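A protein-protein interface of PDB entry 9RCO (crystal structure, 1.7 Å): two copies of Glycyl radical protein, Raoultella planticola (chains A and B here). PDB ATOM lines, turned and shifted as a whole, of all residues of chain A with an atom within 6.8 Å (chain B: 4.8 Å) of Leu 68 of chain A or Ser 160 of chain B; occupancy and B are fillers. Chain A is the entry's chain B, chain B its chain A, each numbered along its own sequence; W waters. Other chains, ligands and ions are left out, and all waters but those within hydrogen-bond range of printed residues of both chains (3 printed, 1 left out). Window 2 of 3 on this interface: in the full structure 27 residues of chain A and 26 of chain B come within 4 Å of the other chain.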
ATOM      1  N   ALA A  61     -18.930  -4.901  13.282  1.00  0.00           N
ATOM      2  CA  ALA A  61     -18.234  -4.894  14.568  1.00  0.00           C
ATOM      3  C   ALA A  61     -18.358  -3.548  15.280  1.00  0.00           C
ATOM      4  O   ALA A  61     -18.468  -3.506  16.514  1.00  0.00           O
ATOM      5  CB  ALA A  61     -16.765  -5.252  14.384  1.00  0.00           C
ATOM      6  N   GLU A  64     -22.035  -3.312  16.570  1.00  0.00           N
ATOM      7  CA  GLU A  64     -22.271  -4.268  17.645  1.00  0.00           C
ATOM      8  C   GLU A  64     -21.627  -3.862  18.966  1.00  0.00           C
ATOM      9  O   GLU A  64     -21.923  -4.484  19.991  1.00  0.00           O
ATOM     10  CB  GLU A  64     -21.731  -5.649  17.246  1.00  0.00           C
ATOM     11  CG  GLU A  64     -22.725  -6.578  16.557  1.00  0.00           C
ATOM     12  CD  GLU A  64     -22.046  -7.647  15.698  1.00  0.00           C
ATOM     13  OE1 GLU A  64     -20.921  -8.089  16.038  1.00  0.00           O
ATOM     14  OE2 GLU A  64     -22.660  -8.067  14.698  1.00  0.00           O
ATOM     15  N   ASN A  65     -20.737  -2.874  18.962  1.00  0.00           N
ATOM     16  CA  ASN A  65     -19.844  -2.621  20.093  1.00  0.00           C
ATOM     17  C   ASN A  65     -19.721  -1.127  20.367  1.00  0.00           C
ATOM     18  O   ASN A  65     -18.634  -0.624  20.682  1.00  0.00           O
ATOM     19  CB  ASN A  65     -18.472  -3.239  19.819  1.00  0.00           C
ATOM     20  CG  ASN A  65     -18.511  -4.751  19.833  1.00  0.00           C
ATOM     21  OD1 ASN A  65     -18.719  -5.365  20.887  1.00  0.00           O
ATOM     22  ND2 ASN A  65     -18.382  -5.363  18.656  1.00  0.00           N
ATOM     23  N   GLU A  66     -20.846  -0.403  20.286  1.00  0.00           N
ATOM     24  CA  GLU A  66     -20.846   1.043  20.499  1.00  0.00           C
ATOM     25  C   GLU A  66     -20.442   1.408  21.916  1.00  0.00           C
ATOM     26  O   GLU A  66     -19.914   2.503  22.147  1.00  0.00           O
ATOM     27  CB  GLU A  66     -22.235   1.618  20.185  1.00  0.00           C
ATOM     28  CG  GLU A  66     -22.593   1.404  18.739  1.00  0.00           C
ATOM     29  CD  GLU A  66     -22.271   2.604  17.866  1.00  0.00           C
ATOM     30  OE1 GLU A  66     -23.162   3.114  17.157  1.00  0.00           O
ATOM     31  OE2 GLU A  66     -21.137   3.101  17.976  1.00  0.00           O
ATOM     32  N   GLN A  67     -20.663   0.502  22.864  1.00  0.00           N
ATOM     33  CA  GLN A  67     -20.495   0.785  24.282  1.00  0.00           C
ATOM     34  C   GLN A  67     -19.059   0.621  24.753  1.00  0.00           C
ATOM     35  O   GLN A  67     -18.740   1.033  25.872  1.00  0.00           O
ATOM     36  CB  GLN A  67     -21.418  -0.135  25.106  1.00  0.00           C
ATOM     37  CG  GLN A  67     -20.839  -1.530  25.356  1.00  0.00           C
ATOM     38  CD  GLN A  67     -21.050  -2.507  24.194  1.00  0.00           C
ATOM     39  OE1 GLN A  67     -21.440  -2.124  23.085  1.00  0.00           O
ATOM     40  NE2 GLN A  67     -20.770  -3.782  24.450  1.00  0.00           N
ATOM     41  N   LEU A  68     -18.183   0.059  23.923  1.00  0.00           N
ATOM     42  CA  LEU A  68     -16.839  -0.237  24.397  1.00  0.00           C
ATOM     43  C   LEU A  68     -15.911   0.970  24.275  1.00  0.00           C
ATOM     44  O   LEU A  68     -16.089   1.816  23.387  1.00  0.00           O
ATOM     45  CB  LEU A  68     -16.243  -1.405  23.597  1.00  0.00           C
ATOM     46  CG  LEU A  68     -16.965  -2.754  23.709  1.00  0.00           C
ATOM     47  CD1 LEU A  68     -16.268  -3.815  22.845  1.00  0.00           C
ATOM     48  CD2 LEU A  68     -17.063  -3.215  25.171  1.00  0.00           C
ATOM     49  N   PRO A  69     -14.887   1.042  25.132  1.00  0.00           N
ATOM     50  CA  PRO A  69     -13.760   1.941  24.850  1.00  0.00           C
ATOM     51  C   PRO A  69     -13.172   1.614  23.487  1.00  0.00           C
ATOM     52  O   PRO A  69     -13.178   0.461  23.048  1.00  0.00           O
ATOM     53  CB  PRO A  69     -12.751   1.627  25.965  1.00  0.00           C
ATOM     54  CG  PRO A  69     -13.500   0.840  26.983  1.00  0.00           C
ATOM     55  CD  PRO A  69     -14.610   0.141  26.266  1.00  0.00           C
ATOM     56  N   ALA A  70     -12.631   2.644  22.832  1.00  0.00           N
ATOM     57  CA  ALA A  70     -12.173   2.486  21.450  1.00  0.00           C
ATOM     58  C   ALA A  70     -11.192   1.325  21.270  1.00  0.00           C
ATOM     59  O   ALA A  70     -11.257   0.603  20.267  1.00  0.00           O
ATOM     60  CB  ALA A  70     -11.540   3.793  20.970  1.00  0.00           C
ATOM     61  N   ILE A  71     -10.259   1.132  22.205  1.00  0.00           N
ATOM     62  CA  ILE A  71      -9.270   0.064  22.000  1.00  0.00           C
ATOM     63  C   ILE A  71      -9.947  -1.307  21.995  1.00  0.00           C
ATOM     64  O   ILE A  71      -9.564  -2.199  21.229  1.00  0.00           O
ATOM     65  CB  ILE A  71      -8.138   0.142  23.045  1.00  0.00           C
ATOM     66  CG1 ILE A  71      -6.972  -0.770  22.649  1.00  0.00           C
ATOM     67  CG2 ILE A  71      -8.660  -0.176  24.467  1.00  0.00           C
ATOM     68  CD1 ILE A  71      -6.089  -0.204  21.505  1.00  0.00           C
ATOM     69  N   MET A  72     -10.988  -1.495  22.817  1.00  0.00           N
ATOM     70  CA  MET A  72     -11.692  -2.775  22.830  1.00  0.00           C
ATOM     71  C   MET A  72     -12.595  -2.918  21.612  1.00  0.00           C
ATOM     72  O   MET A  72     -12.740  -4.018  21.067  1.00  0.00           O
ATOM     73  CB  MET A  72     -12.504  -2.926  24.119  1.00  0.00           C
ATOM     74  CG  MET A  72     -12.982  -4.342  24.400  1.00  0.00           C
ATOM     75  SD  MET A  72     -11.649  -5.562  24.407  1.00  0.00           S
ATOM     76  CE  MET A  72     -11.192  -5.519  26.131  1.00  0.00           C
ATOM     77  N   ARG A  73     -13.207  -1.816  21.180  1.00  0.00           N
ATOM     78  CA  ARG A  73     -13.937  -1.850  19.922  1.00  0.00           C
ATOM     79  C   ARG A  73     -13.027  -2.291  18.785  1.00  0.00           C
ATOM     80  O   ARG A  73     -13.431  -3.084  17.930  1.00  0.00           O
ATOM     81  CB  ARG A  73     -14.527  -0.481  19.618  1.00  0.00           C
ATOM     82  CG  ARG A  73     -15.164  -0.387  18.237  1.00  0.00           C
ATOM     83  CD  ARG A  73     -15.797   0.983  18.063  1.00  0.00           C
ATOM     84  NE  ARG A  73     -16.680   1.232  19.181  1.00  0.00           N
ATOM     85  CZ  ARG A  73     -16.503   2.189  20.082  1.00  0.00           C
ATOM     86  NH1 ARG A  73     -15.490   3.047  19.987  1.00  0.00           N
ATOM     87  NH2 ARG A  73     -17.368   2.296  21.073  1.00  0.00           N
ATOM     88  N   ARG A  74     -11.796  -1.775  18.753  1.00  0.00           N
ATOM     89  CA  ARG A  74     -10.876  -2.146  17.680  1.00  0.00           C
ATOM     90  C   ARG A  74     -10.422  -3.590  17.801  1.00  0.00           C
ATOM     91  O   ARG A  74     -10.129  -4.229  16.782  1.00  0.00           O
ATOM     92  CB  ARG A  74      -9.672  -1.206  17.668  1.00  0.00           C
ATOM     93  CG  ARG A  74     -10.009   0.190  17.162  1.00  0.00           C
ATOM     94  CD  ARG A  74     -10.467   0.186  15.700  1.00  0.00           C
ATOM     95  NE  ARG A  74      -9.573  -0.615  14.872  1.00  0.00           N
ATOM     96  CZ  ARG A  74      -9.693  -0.759  13.555  1.00  0.00           C
ATOM     97  NH1 ARG A  74     -10.668  -0.140  12.910  1.00  0.00           N
ATOM     98  NH2 ARG A  74      -8.828  -1.503  12.890  1.00  0.00           N
ATOM     99  N   LYS A  76     -12.509  -5.941  18.879  1.00  0.00           N
ATOM    100  CA  LYS A  76     -13.669  -6.620  18.302  1.00  0.00           C
ATOM    101  C   LYS A  76     -13.673  -6.539  16.779  1.00  0.00           C
ATOM    102  O   LYS A  76     -14.155  -7.462  16.101  1.00  0.00           O
ATOM    103  CB  LYS A  76     -14.952  -6.007  18.861  1.00  0.00           C
ATOM    104  CG  LYS A  76     -15.188  -6.303  20.330  1.00  0.00           C
ATOM    105  CD  LYS A  76     -15.537  -7.768  20.442  1.00  0.00           C
ATOM    106  CE  LYS A  76     -16.001  -8.171  21.798  1.00  0.00           C
ATOM    107  NZ  LYS A  76     -16.362  -9.619  21.729  1.00  0.00           N
ATOM    108  N   GLN A 226      -7.836  -2.306  29.932  1.00  0.00           N
ATOM    109  CA  GLN A 226      -8.601  -2.367  28.684  1.00  0.00           C
ATOM    110  C   GLN A 226      -7.690  -2.639  27.493  1.00  0.00           C
ATOM    111  O   GLN A 226      -8.015  -3.461  26.632  1.00  0.00           O
ATOM    112  CB  GLN A 226      -9.365  -1.066  28.441  1.00  0.00           C
ATOM    113  CG  GLN A 226     -10.527  -0.846  29.374  1.00  0.00           C
ATOM    114  CD  GLN A 226     -11.613  -1.880  29.157  1.00  0.00           C
ATOM    115  OE1 GLN A 226     -12.001  -2.152  28.019  1.00  0.00           O
ATOM    116  NE2 GLN A 226     -12.073  -2.491  30.236  1.00  0.00           N
ATOM    117  N   SER B 156     -23.341   2.945  29.657  1.00  0.00           N
ATOM    118  CA  SER B 156     -22.885   1.765  28.923  1.00  0.00           C
ATOM    119  C   SER B 156     -21.366   1.730  28.811  1.00  0.00           C
ATOM    120  O   SER B 156     -20.761   0.661  28.915  1.00  0.00           O
ATOM    121  CB  SER B 156     -23.543   1.713  27.541  1.00  0.00           C
ATOM    122  OG  SER B 156     -23.052   2.770  26.735  1.00  0.00           O
ATOM    123  N   LEU B 157     -20.732   2.895  28.646  1.00  0.00           N
ATOM    124  CA  LEU B 157     -19.270   2.955  28.636  1.00  0.00           C
ATOM    125  C   LEU B 157     -18.681   2.666  30.013  1.00  0.00           C
ATOM    126  O   LEU B 157     -17.690   1.927  30.128  1.00  0.00           O
ATOM    127  CB  LEU B 157     -18.805   4.327  28.142  1.00  0.00           C
ATOM    128  CG  LEU B 157     -17.282   4.516  28.141  1.00  0.00           C
ATOM    129  CD1 LEU B 157     -16.581   3.520  27.206  1.00  0.00           C
ATOM    130  CD2 LEU B 157     -16.906   5.964  27.781  1.00  0.00           C
ATOM    131  N   ALA B 158     -19.253   3.269  31.067  1.00  0.00           N
ATOM    132  CA  ALA B 158     -18.768   3.044  32.428  1.00  0.00           C
ATOM    133  C   ALA B 158     -18.757   1.560  32.773  1.00  0.00           C
ATOM    134  O   ALA B 158     -17.780   1.047  33.336  1.00  0.00           O
ATOM    135  CB  ALA B 158     -19.640   3.817  33.429  1.00  0.00           C
ATOM    136  N   ALA B 159     -19.842   0.853  32.456  1.00  0.00           N
ATOM    137  CA  ALA B 159     -19.907  -0.567  32.788  1.00  0.00           C
ATOM    138  C   ALA B 159     -18.822  -1.353  32.061  1.00  0.00           C
ATOM    139  O   ALA B 159     -18.283  -2.324  32.607  1.00  0.00           O
ATOM    140  CB  ALA B 159     -21.290  -1.127  32.442  1.00  0.00           C
ATOM    141  N   SER B 160     -18.470  -0.928  30.844  1.00  0.00           N
ATOM    142  CA  SER B 160     -17.451  -1.625  30.064  1.00  0.00           C
ATOM    143  C   SER B 160     -16.064  -1.495  30.670  1.00  0.00           C
ATOM    144  O   SER B 160     -15.203  -2.334  30.399  1.00  0.00           O
ATOM    145  CB  SER B 160     -17.427  -1.100  28.626  1.00  0.00           C
ATOM    146  OG  SER B 160     -18.668  -1.333  27.987  1.00  0.00           O
ATOM    147  N   TYR B 161     -15.821  -0.450  31.460  1.00  0.00           N
ATOM    148  CA  TYR B 161     -14.517  -0.277  32.085  1.00  0.00           C
ATOM    149  C   TYR B 161     -14.361  -1.104  33.353  1.00  0.00           C
ATOM    150  O   TYR B 161     -13.228  -1.352  33.776  1.00  0.00           O
ATOM    151  CB  TYR B 161     -14.265   1.201  32.420  1.00  0.00           C
ATOM    152  CG  TYR B 161     -13.724   2.046  31.260  1.00  0.00           C
ATOM    153  CD1 TYR B 161     -12.506   1.735  30.663  1.00  0.00           C
ATOM    154  CD2 TYR B 161     -14.416   3.177  30.800  1.00  0.00           C
ATOM    155  CE1 TYR B 161     -11.994   2.509  29.626  1.00  0.00           C
ATOM    156  CE2 TYR B 161     -13.910   3.962  29.758  1.00  0.00           C
ATOM    157  CZ  TYR B 161     -12.696   3.617  29.177  1.00  0.00           C
ATOM    158  OH  TYR B 161     -12.161   4.364  28.152  1.00  0.00           O
ATOM    159  N   MET B 162     -15.465  -1.532  33.960  1.00  0.00           N
ATOM    160  CA  MET B 162     -15.432  -2.206  35.249  1.00  0.00           C
ATOM    161  C   MET B 162     -15.119  -3.691  35.106  1.00  0.00           C
ATOM    162  O   MET B 162     -15.555  -4.351  34.155  1.00  0.00           O
ATOM    163  CB  MET B 162     -16.776  -2.066  35.943  1.00  0.00           C
ATOM    164  CG  MET B 162     -17.223  -0.643  36.140  1.00  0.00           C
ATOM    165  SD  MET B 162     -18.824  -0.669  36.940  1.00  0.00           S
ATOM    166  CE  MET B 162     -19.278   1.073  36.842  1.00  0.00           C
ATOM    167  N   ARG B 539     -17.221  11.002  27.452  1.00  0.00           N
ATOM    168  CA  ARG B 539     -18.439  11.139  26.665  1.00  0.00           C
ATOM    169  C   ARG B 539     -19.292  12.356  27.006  1.00  0.00           C
ATOM    170  O   ARG B 539     -20.088  12.777  26.158  1.00  0.00           O
ATOM    171  CB  ARG B 539     -19.310   9.878  26.797  1.00  0.00           C
ATOM    172  CG  ARG B 539     -18.734   8.670  26.057  1.00  0.00           C
ATOM    173  CD  ARG B 539     -19.739   7.511  25.924  1.00  0.00           C
ATOM    174  NE  ARG B 539     -19.197   6.544  24.971  1.00  0.00           N
ATOM    175  CZ  ARG B 539     -19.803   5.430  24.578  1.00  0.00           C
ATOM    176  NH1 ARG B 539     -20.993   5.092  25.063  1.00  0.00           N
ATOM    177  NH2 ARG B 539     -19.197   4.644  23.693  1.00  0.00           N
HETATM  178  O   HOH W   1     -10.680  -1.732  32.565  1.00  0.00           O
HETATM  179  O   HOH W   2     -16.437   4.447  22.705  1.00  0.00           O
HETATM  180  O   HOH W   3     -20.111   4.526  20.349  1.00  0.00           O
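No position is printed for both chains.
Of the 12 pairs that touch across the chains among the printed residues, none has its exchanged pair printed and touching as well.
Water W3 bridges O of Glu 66 of chain A and NH2 of Arg 539 of chain B.
Water W2 lies within hydrogen-bond range of O of Leu 68 of chain A (2.7 Å), NH2 of Arg 73 of chain A (2.9 Å) and NH2 of Arg 539 of chain B (2.9 Å).
Water W1 lies within hydrogen-bond range of the side-chain amide nitrogen (NE2) of Gln 226 of chain A and the backbone carbonyl oxygen (O) of Tyr 161 of chain B.
Of the 14 printed residues of chain A, 6 touch a printed residue of chain B.
Hydrophobic or aromatic side chains of chain A within 4 Å of the printed part of chain B: Leu 68 and Pro 69.
Along chain A the printed residues that touch a printed residue of chain B span positions 66 to 226.
Of the 8 printed residues of chain B, 5 touch a printed residue of chain A.
Printed residues of chain B that touch a printed residue of chain A: Ser 156, Leu 157, Ser 160, Tyr 161 and Arg 539.
Hydrophobic or aromatic side chains of chain B that line the printed part of chain A: Leu 157 and Tyr 161.
Among the printed residues, no Asp or Glu carboxylate lies within 4 Å of a Lys or Arg side-chain nitrogen of the other chain.
Of the printed residues of chain B, Gln 67 of chain A touches Ser 156, Leu 157 and Ser 160.
Of the printed residues of chain B, Leu 68 of chain A touches Leu 157 (3.9 Å) and Ser 160 (3.7 Å).
Of the printed residues of chain A, Ser 156 of chain B touches Gln 67 (3.7 Å).
Of chain A, only Gln 67, Leu 68, Pro 69 and Gln 226 come within 4 Å of Ser 160 of chain B.
The nearest printed residue of chain A that does not touch Ser 160 of chain B is Met 72 of chain A (6.7 Å).
O of Ser 156 of chain B sits at hydrogen-bond distance from OG of Ser 160 of chain B (3.0 Å).
O of Asn 65 of chain A is in hydrogen-bond range of NE of Arg 73 of chain A, 3.1 Å away.
The guanidinium group (NH2) of Arg 73 of chain A lies within hydrogen-bond range of the backbone carbonyl oxygen (O) of Glu 66 of chain A, at 2.8 Å.
The backbone carbonyl oxygen of Leu 68 of chain A lies within hydrogen-bond range of the guanidinium group of Arg 73 of chain A, 2.7 Å away.
The side-chain hydroxyl (OG) of Ser 160 of chain B is in hydrogen-bond range of the backbone carbonyl oxygen (O) of Gln 67 of chain A, at 3.2 Å.
The backbone carbonyl oxygen of Ser 160 of chain B is in hydrogen-bond range of the side-chain amide nitrogen of Gln 226 of chain A (3.1 Å).
O of Glu 66 of chain A lies within hydrogen-bond range of NH2 of Arg 539 of chain B, 2.7 Å away.
O of Ser 156 of chain B touches O of Gln 67 of chain A, at 3.7 Å.
O of Gln 67 of chain A touches CA of Leu 157 of chain B, 3.4 Å away.
CD1 of Leu 157 of chain B touches C of Leu 68 of chain A (3.9 Å).
CD2 of Leu 68 of chain A touches OG of Ser 160 of chain B, 3.7 Å away.
N of Pro 69 of chain A touches CD1 of Leu 157 of chain B, 3.6 Å away.
Pro 69 of chain A touches Ser 160 of chain B.
Tyr 161 of chain B touches Pro 69 of chain A.
Arg 73 of chain A touches Arg 539 of chain B (NH2 to NH2, 3.97 Å).
Tyr 161 of chain B touches Gln 226 of chain A.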
